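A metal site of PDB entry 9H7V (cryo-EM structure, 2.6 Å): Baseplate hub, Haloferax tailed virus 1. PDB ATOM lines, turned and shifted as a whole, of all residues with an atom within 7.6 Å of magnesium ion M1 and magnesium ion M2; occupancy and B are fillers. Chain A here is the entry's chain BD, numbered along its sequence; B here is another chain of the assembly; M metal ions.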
ATOM      1  N   VAL A  44      22.721   2.268   9.354  1.00  0.00           N
ATOM      2  CA  VAL A  44      24.170   2.381   9.441  1.00  0.00           C
ATOM      3  C   VAL A  44      24.647   3.458   8.474  1.00  0.00           C
ATOM      4  O   VAL A  44      24.320   3.434   7.291  1.00  0.00           O
ATOM      5  CB  VAL A  44      24.873   1.027   9.217  1.00  0.00           C
ATOM      6  CG1 VAL A  44      26.391   1.148   9.314  1.00  0.00           C
ATOM      7  CG2 VAL A  44      24.379  -0.033  10.189  1.00  0.00           C
ATOM      8  N   ASP A  45      25.431   4.401   9.019  1.00  0.00           N
ATOM      9  CA  ASP A  45      26.025   5.510   8.287  1.00  0.00           C
ATOM     10  C   ASP A  45      27.528   5.456   8.502  1.00  0.00           C
ATOM     11  O   ASP A  45      27.989   5.585   9.629  1.00  0.00           O
ATOM     12  CB  ASP A  45      25.408   6.833   8.769  1.00  0.00           C
ATOM     13  CG  ASP A  45      25.735   8.052   7.924  1.00  0.00           C
ATOM     14  OD1 ASP A  45      26.386   7.886   6.864  1.00  0.00           O
ATOM     15  OD2 ASP A  45      25.340   9.161   8.326  1.00  0.00           O
ATOM     16  N   THR A  46      28.289   5.255   7.408  1.00  0.00           N
ATOM     17  CA  THR A  46      29.682   4.836   7.542  1.00  0.00           C
ATOM     18  C   THR A  46      30.556   5.385   6.410  1.00  0.00           C
ATOM     19  O   THR A  46      30.123   5.449   5.252  1.00  0.00           O
ATOM     20  CB  THR A  46      29.788   3.322   7.752  1.00  0.00           C
ATOM     21  OG1 THR A  46      31.163   2.950   7.886  1.00  0.00           O
ATOM     22  CG2 THR A  46      29.133   2.504   6.649  1.00  0.00           C
ATOM     23  N   ALA A  47      31.799   5.720   6.785  1.00  0.00           N
ATOM     24  CA  ALA A  47      32.821   6.339   5.942  1.00  0.00           C
ATOM     25  C   ALA A  47      33.162   5.447   4.747  1.00  0.00           C
ATOM     26  O   ALA A  47      32.847   4.253   4.746  1.00  0.00           O
ATOM     27  CB  ALA A  47      34.039   6.657   6.775  1.00  0.00           C
ATOM     28  N   ASN A  48      33.882   6.036   3.781  1.00  0.00           N
ATOM     29  CA  ASN A  48      33.837   5.679   2.368  1.00  0.00           C
ATOM     30  C   ASN A  48      34.101   4.199   2.065  1.00  0.00           C
ATOM     31  O   ASN A  48      33.380   3.664   1.225  1.00  0.00           O
ATOM     32  CB  ASN A  48      34.645   6.650   1.497  1.00  0.00           C
ATOM     33  CG  ASN A  48      33.964   7.989   1.363  1.00  0.00           C
ATOM     34  OD1 ASN A  48      32.874   8.083   0.795  1.00  0.00           O
ATOM     35  ND2 ASN A  48      34.595   9.019   1.889  1.00  0.00           N
ATOM     36  N   PRO A  49      35.106   3.503   2.655  1.00  0.00           N
ATOM     37  CA  PRO A  49      35.324   2.086   2.326  1.00  0.00           C
ATOM     38  C   PRO A  49      34.100   1.185   2.531  1.00  0.00           C
ATOM     39  O   PRO A  49      34.052   0.084   1.995  1.00  0.00           O
ATOM     40  CB  PRO A  49      36.451   1.660   3.275  1.00  0.00           C
ATOM     41  CG  PRO A  49      37.178   2.946   3.587  1.00  0.00           C
ATOM     42  CD  PRO A  49      36.102   4.010   3.611  1.00  0.00           C
ATOM     43  N   PHE A  50      33.106   1.694   3.277  1.00  0.00           N
ATOM     44  CA  PHE A  50      32.008   0.879   3.786  1.00  0.00           C
ATOM     45  C   PHE A  50      30.650   1.417   3.313  1.00  0.00           C
ATOM     46  O   PHE A  50      30.450   2.625   3.232  1.00  0.00           O
ATOM     47  CB  PHE A  50      32.073   0.785   5.305  1.00  0.00           C
ATOM     48  CG  PHE A  50      33.330   0.130   5.828  1.00  0.00           C
ATOM     49  CD1 PHE A  50      33.443  -1.251   5.868  1.00  0.00           C
ATOM     50  CD2 PHE A  50      34.397   0.899   6.258  1.00  0.00           C
ATOM     51  CE1 PHE A  50      34.596  -1.848   6.336  1.00  0.00           C
ATOM     52  CE2 PHE A  50      35.557   0.296   6.730  1.00  0.00           C
ATOM     53  CZ  PHE A  50      35.654  -1.089   6.770  1.00  0.00           C
ATOM     54  N   GLY A  51      29.734   0.475   3.049  1.00  0.00           N
ATOM     55  CA  GLY A  51      28.425   0.774   2.511  1.00  0.00           C
ATOM     56  C   GLY A  51      27.420   1.163   3.600  1.00  0.00           C
ATOM     57  O   GLY A  51      27.284   0.455   4.593  1.00  0.00           O
ATOM     58  N   ASP A  52      26.738   2.296   3.387  1.00  0.00           N
ATOM     59  CA  ASP A  52      25.628   2.724   4.219  1.00  0.00           C
ATOM     60  C   ASP A  52      24.422   1.845   3.901  1.00  0.00           C
ATOM     61  O   ASP A  52      24.091   1.650   2.733  1.00  0.00           O
ATOM     62  CB  ASP A  52      25.295   4.197   3.995  1.00  0.00           C
ATOM     63  CG  ASP A  52      26.428   5.173   4.252  1.00  0.00           C
ATOM     64  OD1 ASP A  52      27.581   4.719   4.437  1.00  0.00           O
ATOM     65  OD2 ASP A  52      26.156   6.384   4.271  1.00  0.00           O
ATOM     66  N   TYR A  53      23.781   1.319   4.949  1.00  0.00           N
ATOM     67  CA  TYR A  53      22.651   0.425   4.763  1.00  0.00           C
ATOM     68  C   TYR A  53      21.606   0.597   5.868  1.00  0.00           C
ATOM     69  O   TYR A  53      21.919   1.095   6.943  1.00  0.00           O
ATOM     70  CB  TYR A  53      23.112  -1.034   4.622  1.00  0.00           C
ATOM     71  CG  TYR A  53      23.578  -1.722   5.888  1.00  0.00           C
ATOM     72  CD1 TYR A  53      24.857  -1.527   6.385  1.00  0.00           C
ATOM     73  CD2 TYR A  53      22.745  -2.594   6.570  1.00  0.00           C
ATOM     74  CE1 TYR A  53      25.294  -2.168   7.532  1.00  0.00           C
ATOM     75  CE2 TYR A  53      23.160  -3.241   7.726  1.00  0.00           C
ATOM     76  CZ  TYR A  53      24.446  -3.029   8.208  1.00  0.00           C
ATOM     77  OH  TYR A  53      24.862  -3.658   9.332  1.00  0.00           O
ATOM     78  N   ARG A  89      16.906  10.531   8.214  1.00  0.00           N
ATOM     79  CA  ARG A  89      18.208  10.049   8.639  1.00  0.00           C
ATOM     80  C   ARG A  89      18.829   9.088   7.626  1.00  0.00           C
ATOM     81  O   ARG A  89      20.052   8.964   7.574  1.00  0.00           O
ATOM     82  CB  ARG A  89      18.150   9.457  10.058  1.00  0.00           C
ATOM     83  CG  ARG A  89      19.513   9.227  10.712  1.00  0.00           C
ATOM     84  CD  ARG A  89      20.396  10.463  10.697  1.00  0.00           C
ATOM     85  NE  ARG A  89      21.798  10.268  11.067  1.00  0.00           N
ATOM     86  CZ  ARG A  89      22.762   9.853  10.251  1.00  0.00           C
ATOM     87  NH1 ARG A  89      23.992   9.722  10.719  1.00  0.00           N
ATOM     88  NH2 ARG A  89      22.507   9.546   8.993  1.00  0.00           N
ATOM     89  N   SER A 114      22.495   2.754  -0.065  1.00  0.00           N
ATOM     90  CA  SER A 114      22.421   4.191  -0.298  1.00  0.00           C
ATOM     91  C   SER A 114      23.354   4.623  -1.433  1.00  0.00           C
ATOM     92  O   SER A 114      23.779   3.798  -2.235  1.00  0.00           O
ATOM     93  CB  SER A 114      22.667   4.955   0.985  1.00  0.00           C
ATOM     94  OG  SER A 114      22.250   6.310   0.858  1.00  0.00           O
ATOM     95  N   PHE A 115      23.659   5.928  -1.484  1.00  0.00           N
ATOM     96  CA  PHE A 115      24.239   6.602  -2.645  1.00  0.00           C
ATOM     97  C   PHE A 115      25.714   6.284  -2.836  1.00  0.00           C
ATOM     98  O   PHE A 115      26.239   6.491  -3.932  1.00  0.00           O
ATOM     99  CB  PHE A 115      24.015   8.113  -2.578  1.00  0.00           C
ATOM    100  CG  PHE A 115      22.561   8.510  -2.474  1.00  0.00           C
ATOM    101  CD1 PHE A 115      21.735   8.456  -3.593  1.00  0.00           C
ATOM    102  CD2 PHE A 115      22.025   8.905  -1.255  1.00  0.00           C
ATOM    103  CE1 PHE A 115      20.394   8.809  -3.487  1.00  0.00           C
ATOM    104  CE2 PHE A 115      20.686   9.251  -1.162  1.00  0.00           C
ATOM    105  CZ  PHE A 115      19.871   9.199  -2.273  1.00  0.00           C
ATOM    106  N   ASP A 116      26.388   5.786  -1.789  1.00  0.00           N
ATOM    107  CA  ASP A 116      27.816   5.512  -1.865  1.00  0.00           C
ATOM    108  C   ASP A 116      28.094   4.331  -2.795  1.00  0.00           C
ATOM    109  O   ASP A 116      29.231   4.122  -3.209  1.00  0.00           O
ATOM    110  CB  ASP A 116      28.511   5.517  -0.490  1.00  0.00           C
ATOM    111  CG  ASP A 116      28.144   4.409   0.479  1.00  0.00           C
ATOM    112  OD1 ASP A 116      27.286   3.568   0.145  1.00  0.00           O
ATOM    113  OD2 ASP A 116      28.731   4.396   1.593  1.00  0.00           O
ATOM    114  N   GLN A 117      27.025   3.591  -3.146  1.00  0.00           N
ATOM    115  CA  GLN A 117      27.079   2.470  -4.075  1.00  0.00           C
ATOM    116  C   GLN A 117      27.473   2.935  -5.474  1.00  0.00           C
ATOM    117  O   GLN A 117      28.114   2.173  -6.201  1.00  0.00           O
ATOM    118  CB  GLN A 117      25.744   1.723  -4.100  1.00  0.00           C
ATOM    119  CG  GLN A 117      25.448   0.915  -2.845  1.00  0.00           C
ATOM    120  CD  GLN A 117      26.443  -0.183  -2.550  1.00  0.00           C
ATOM    121  OE1 GLN A 117      26.982  -0.825  -3.438  1.00  0.00           O
ATOM    122  NE2 GLN A 117      26.690  -0.408  -1.263  1.00  0.00           N
ATOM    123  N   ARG A 120      31.127   3.422  -5.935  1.00  0.00           N
ATOM    124  CA  ARG A 120      31.768   2.142  -5.676  1.00  0.00           C
ATOM    125  C   ARG A 120      31.686   1.249  -6.920  1.00  0.00           C
ATOM    126  O   ARG A 120      32.640   0.545  -7.239  1.00  0.00           O
ATOM    127  CB  ARG A 120      31.027   1.493  -4.506  1.00  0.00           C
ATOM    128  CG  ARG A 120      31.729   0.303  -3.852  1.00  0.00           C
ATOM    129  CD  ARG A 120      31.144   0.027  -2.482  1.00  0.00           C
ATOM    130  NE  ARG A 120      31.446   1.107  -1.547  1.00  0.00           N
ATOM    131  CZ  ARG A 120      30.582   1.716  -0.738  1.00  0.00           C
ATOM    132  NH1 ARG A 120      30.997   2.683   0.058  1.00  0.00           N
ATOM    133  NH2 ARG A 120      29.306   1.345  -0.701  1.00  0.00           N
ATOM    134  N   GLU A 172      35.640   5.304  -6.189  1.00  0.00           N
ATOM    135  CA  GLU A 172      35.907   5.401  -4.756  1.00  0.00           C
ATOM    136  C   GLU A 172      37.387   5.180  -4.452  1.00  0.00           C
ATOM    137  O   GLU A 172      37.942   5.852  -3.577  1.00  0.00           O
ATOM    138  CB  GLU A 172      35.000   4.423  -4.003  1.00  0.00           C
ATOM    139  CG  GLU A 172      35.062   4.548  -2.490  1.00  0.00           C
ATOM    140  CD  GLU A 172      34.463   3.346  -1.786  1.00  0.00           C
ATOM    141  OE1 GLU A 172      33.225   3.245  -1.728  1.00  0.00           O
ATOM    142  OE2 GLU A 172      35.253   2.488  -1.319  1.00  0.00           O
ATOM    143  N   PHE A 187      35.193  12.663   1.566  1.00  0.00           N
ATOM    144  CA  PHE A 187      34.358  12.760   0.370  1.00  0.00           C
ATOM    145  C   PHE A 187      33.092  11.931   0.553  1.00  0.00           C
ATOM    146  O   PHE A 187      32.976  11.146   1.491  1.00  0.00           O
ATOM    147  CB  PHE A 187      35.150  12.391  -0.894  1.00  0.00           C
ATOM    148  CG  PHE A 187      35.632  10.967  -0.963  1.00  0.00           C
ATOM    149  CD1 PHE A 187      34.853   9.979  -1.565  1.00  0.00           C
ATOM    150  CD2 PHE A 187      36.867  10.608  -0.452  1.00  0.00           C
ATOM    151  CE1 PHE A 187      35.305   8.673  -1.636  1.00  0.00           C
ATOM    152  CE2 PHE A 187      37.313   9.299  -0.516  1.00  0.00           C
ATOM    153  CZ  PHE A 187      36.535   8.333  -1.112  1.00  0.00           C
ATOM    154  N   GLY A 188      32.146  12.137  -0.369  1.00  0.00           N
ATOM    155  CA  GLY A 188      30.922  11.352  -0.405  1.00  0.00           C
ATOM    156  C   GLY A 188      29.791  12.099  -1.103  1.00  0.00           C
ATOM    157  O   GLY A 188      30.010  13.133  -1.735  1.00  0.00           O
ATOM    158  N   VAL A 189      28.585  11.546  -0.968  1.00  0.00           N
ATOM    159  CA  VAL A 189      27.371  12.126  -1.506  1.00  0.00           C
ATOM    160  C   VAL A 189      26.535  12.600  -0.319  1.00  0.00           C
ATOM    161  O   VAL A 189      26.199  11.815   0.570  1.00  0.00           O
ATOM    162  CB  VAL A 189      26.597  11.119  -2.380  1.00  0.00           C
ATOM    163  CG1 VAL A 189      25.378  11.744  -3.033  1.00  0.00           C
ATOM    164  CG2 VAL A 189      27.482  10.477  -3.430  1.00  0.00           C
ATOM    165  N   ASP A 191      23.029  14.526   1.451  1.00  0.00           N
ATOM    166  CA  ASP A 191      21.605  14.247   1.412  1.00  0.00           C
ATOM    167  C   ASP A 191      20.957  14.899   0.189  1.00  0.00           C
ATOM    168  O   ASP A 191      19.932  14.432  -0.296  1.00  0.00           O
ATOM    169  CB  ASP A 191      20.917  14.699   2.705  1.00  0.00           C
ATOM    170  CG  ASP A 191      21.401  14.016   3.971  1.00  0.00           C
ATOM    171  OD1 ASP A 191      21.933  12.885   3.875  1.00  0.00           O
ATOM    172  OD2 ASP A 191      21.248  14.614   5.055  1.00  0.00           O
ATOM    173  N   PHE A 196      30.755  15.965  -2.391  1.00  0.00           N
ATOM    174  CA  PHE A 196      31.645  16.845  -1.657  1.00  0.00           C
ATOM    175  C   PHE A 196      33.033  16.215  -1.544  1.00  0.00           C
ATOM    176  O   PHE A 196      33.159  14.995  -1.553  1.00  0.00           O
ATOM    177  CB  PHE A 196      31.066  17.222  -0.286  1.00  0.00           C
ATOM    178  CG  PHE A 196      30.934  16.078   0.696  1.00  0.00           C
ATOM    179  CD1 PHE A 196      31.978  15.743   1.540  1.00  0.00           C
ATOM    180  CD2 PHE A 196      29.753  15.358   0.792  1.00  0.00           C
ATOM    181  CE1 PHE A 196      31.859  14.689   2.443  1.00  0.00           C
ATOM    182  CE2 PHE A 196      29.626  14.310   1.692  1.00  0.00           C
ATOM    183  CZ  PHE A 196      30.681  13.979   2.520  1.00  0.00           C
ATOM    184  N   GLU A 307      27.124  12.608  12.137  1.00  0.00           N
ATOM    185  CA  GLU A 307      27.532  11.940  10.910  1.00  0.00           C
ATOM    186  C   GLU A 307      28.955  11.408  11.083  1.00  0.00           C
ATOM    187  O   GLU A 307      29.670  11.873  11.963  1.00  0.00           O
ATOM    188  CB  GLU A 307      27.470  12.912   9.742  1.00  0.00           C
ATOM    189  CG  GLU A 307      26.061  13.184   9.227  1.00  0.00           C
ATOM    190  CD  GLU A 307      25.966  14.120   8.040  1.00  0.00           C
ATOM    191  OE1 GLU A 307      26.852  14.056   7.165  1.00  0.00           O
ATOM    192  OE2 GLU A 307      25.007  14.912   7.998  1.00  0.00           O
ATOM    193  N   PRO A 308      29.414  10.425  10.264  1.00  0.00           N
ATOM    194  CA  PRO A 308      30.841  10.108  10.176  1.00  0.00           C
ATOM    195  C   PRO A 308      31.604  11.302   9.627  1.00  0.00           C
ATOM    196  O   PRO A 308      31.136  11.995   8.719  1.00  0.00           O
ATOM    197  CB  PRO A 308      30.919   8.892   9.239  1.00  0.00           C
ATOM    198  CG  PRO A 308      29.608   8.917   8.481  1.00  0.00           C
ATOM    199  CD  PRO A 308      28.600   9.529   9.429  1.00  0.00           C
ATOM    200  N   ALA A 328      33.894   7.404  12.809  1.00  0.00           N
ATOM    201  CA  ALA A 328      34.123   6.647  11.586  1.00  0.00           C
ATOM    202  C   ALA A 328      32.811   6.065  11.066  1.00  0.00           C
ATOM    203  O   ALA A 328      32.631   5.935   9.854  1.00  0.00           O
ATOM    204  CB  ALA A 328      35.141   5.573  11.842  1.00  0.00           C
ATOM    205  N   ARG B 338      27.969  -5.200   0.325  1.00  0.00           N
ATOM    206  CA  ARG B 338      27.923  -3.777   0.586  1.00  0.00           C
ATOM    207  C   ARG B 338      29.111  -3.061  -0.047  1.00  0.00           C
ATOM    208  O   ARG B 338      29.024  -1.877  -0.354  1.00  0.00           O
ATOM    209  CB  ARG B 338      27.898  -3.520   2.099  1.00  0.00           C
ATOM    210  CG  ARG B 338      26.509  -3.235   2.659  1.00  0.00           C
ATOM    211  CD  ARG B 338      26.215  -3.979   3.956  1.00  0.00           C
ATOM    212  NE  ARG B 338      27.184  -3.738   5.021  1.00  0.00           N
ATOM    213  CZ  ARG B 338      27.265  -4.431   6.151  1.00  0.00           C
ATOM    214  NH1 ARG B 338      28.179  -4.115   7.051  1.00  0.00           N
ATOM    215  NH2 ARG B 338      26.429  -5.434   6.393  1.00  0.00           N
HETATM  216 MG    MG M   1      29.434   4.461   3.481  1.00  0.00          MG
HETATM  217 MG    MG M   2      27.448   8.375   4.945  1.00  0.00          MG
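Magnesium ion M1 is bound by OD2 of Asp 116 (2.0 Å), OD1 of Asp 52 (2.1 Å), O of Phe 50 (2.1 Å) and O of Thr 46 (2.1 Å).
Magnesium ion M1 has four donor atoms within binding distance.
Merely in contact with magnesium ion M1: Ala 47 and Gly 51.
O of Phe 50 sits close to NH1 of Arg 120, 3.2 Å away.
The backbone carbonyl oxygen (O) of Asp 52 lies within hydrogen-bond range of the backbone NH (N) of Ser 114, 3.4 Å away.
N of Ala 47 is in hydrogen-bond range of O of Ala 328 (3.2 Å).
The guanidinium group (NH2) of Arg 120 lies within salt-bridge range of the side-chain carboxylate (OD1) of Asp 116 (3.1 Å).
The guanidinium group (NH1) of Arg 89 is in salt-bridge range of the side-chain carboxylate (OD2) of Asp 45 (2.8 Å).
Magnesium ion M2 is bound by the side-chain carboxylate of Asp 45 (2.2 Å) and the side-chain carboxylate of Asp 52 (2.5 Å).
Within 4 Å of magnesium ion M2: Asp 45, Thr 46 and Asp 52.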
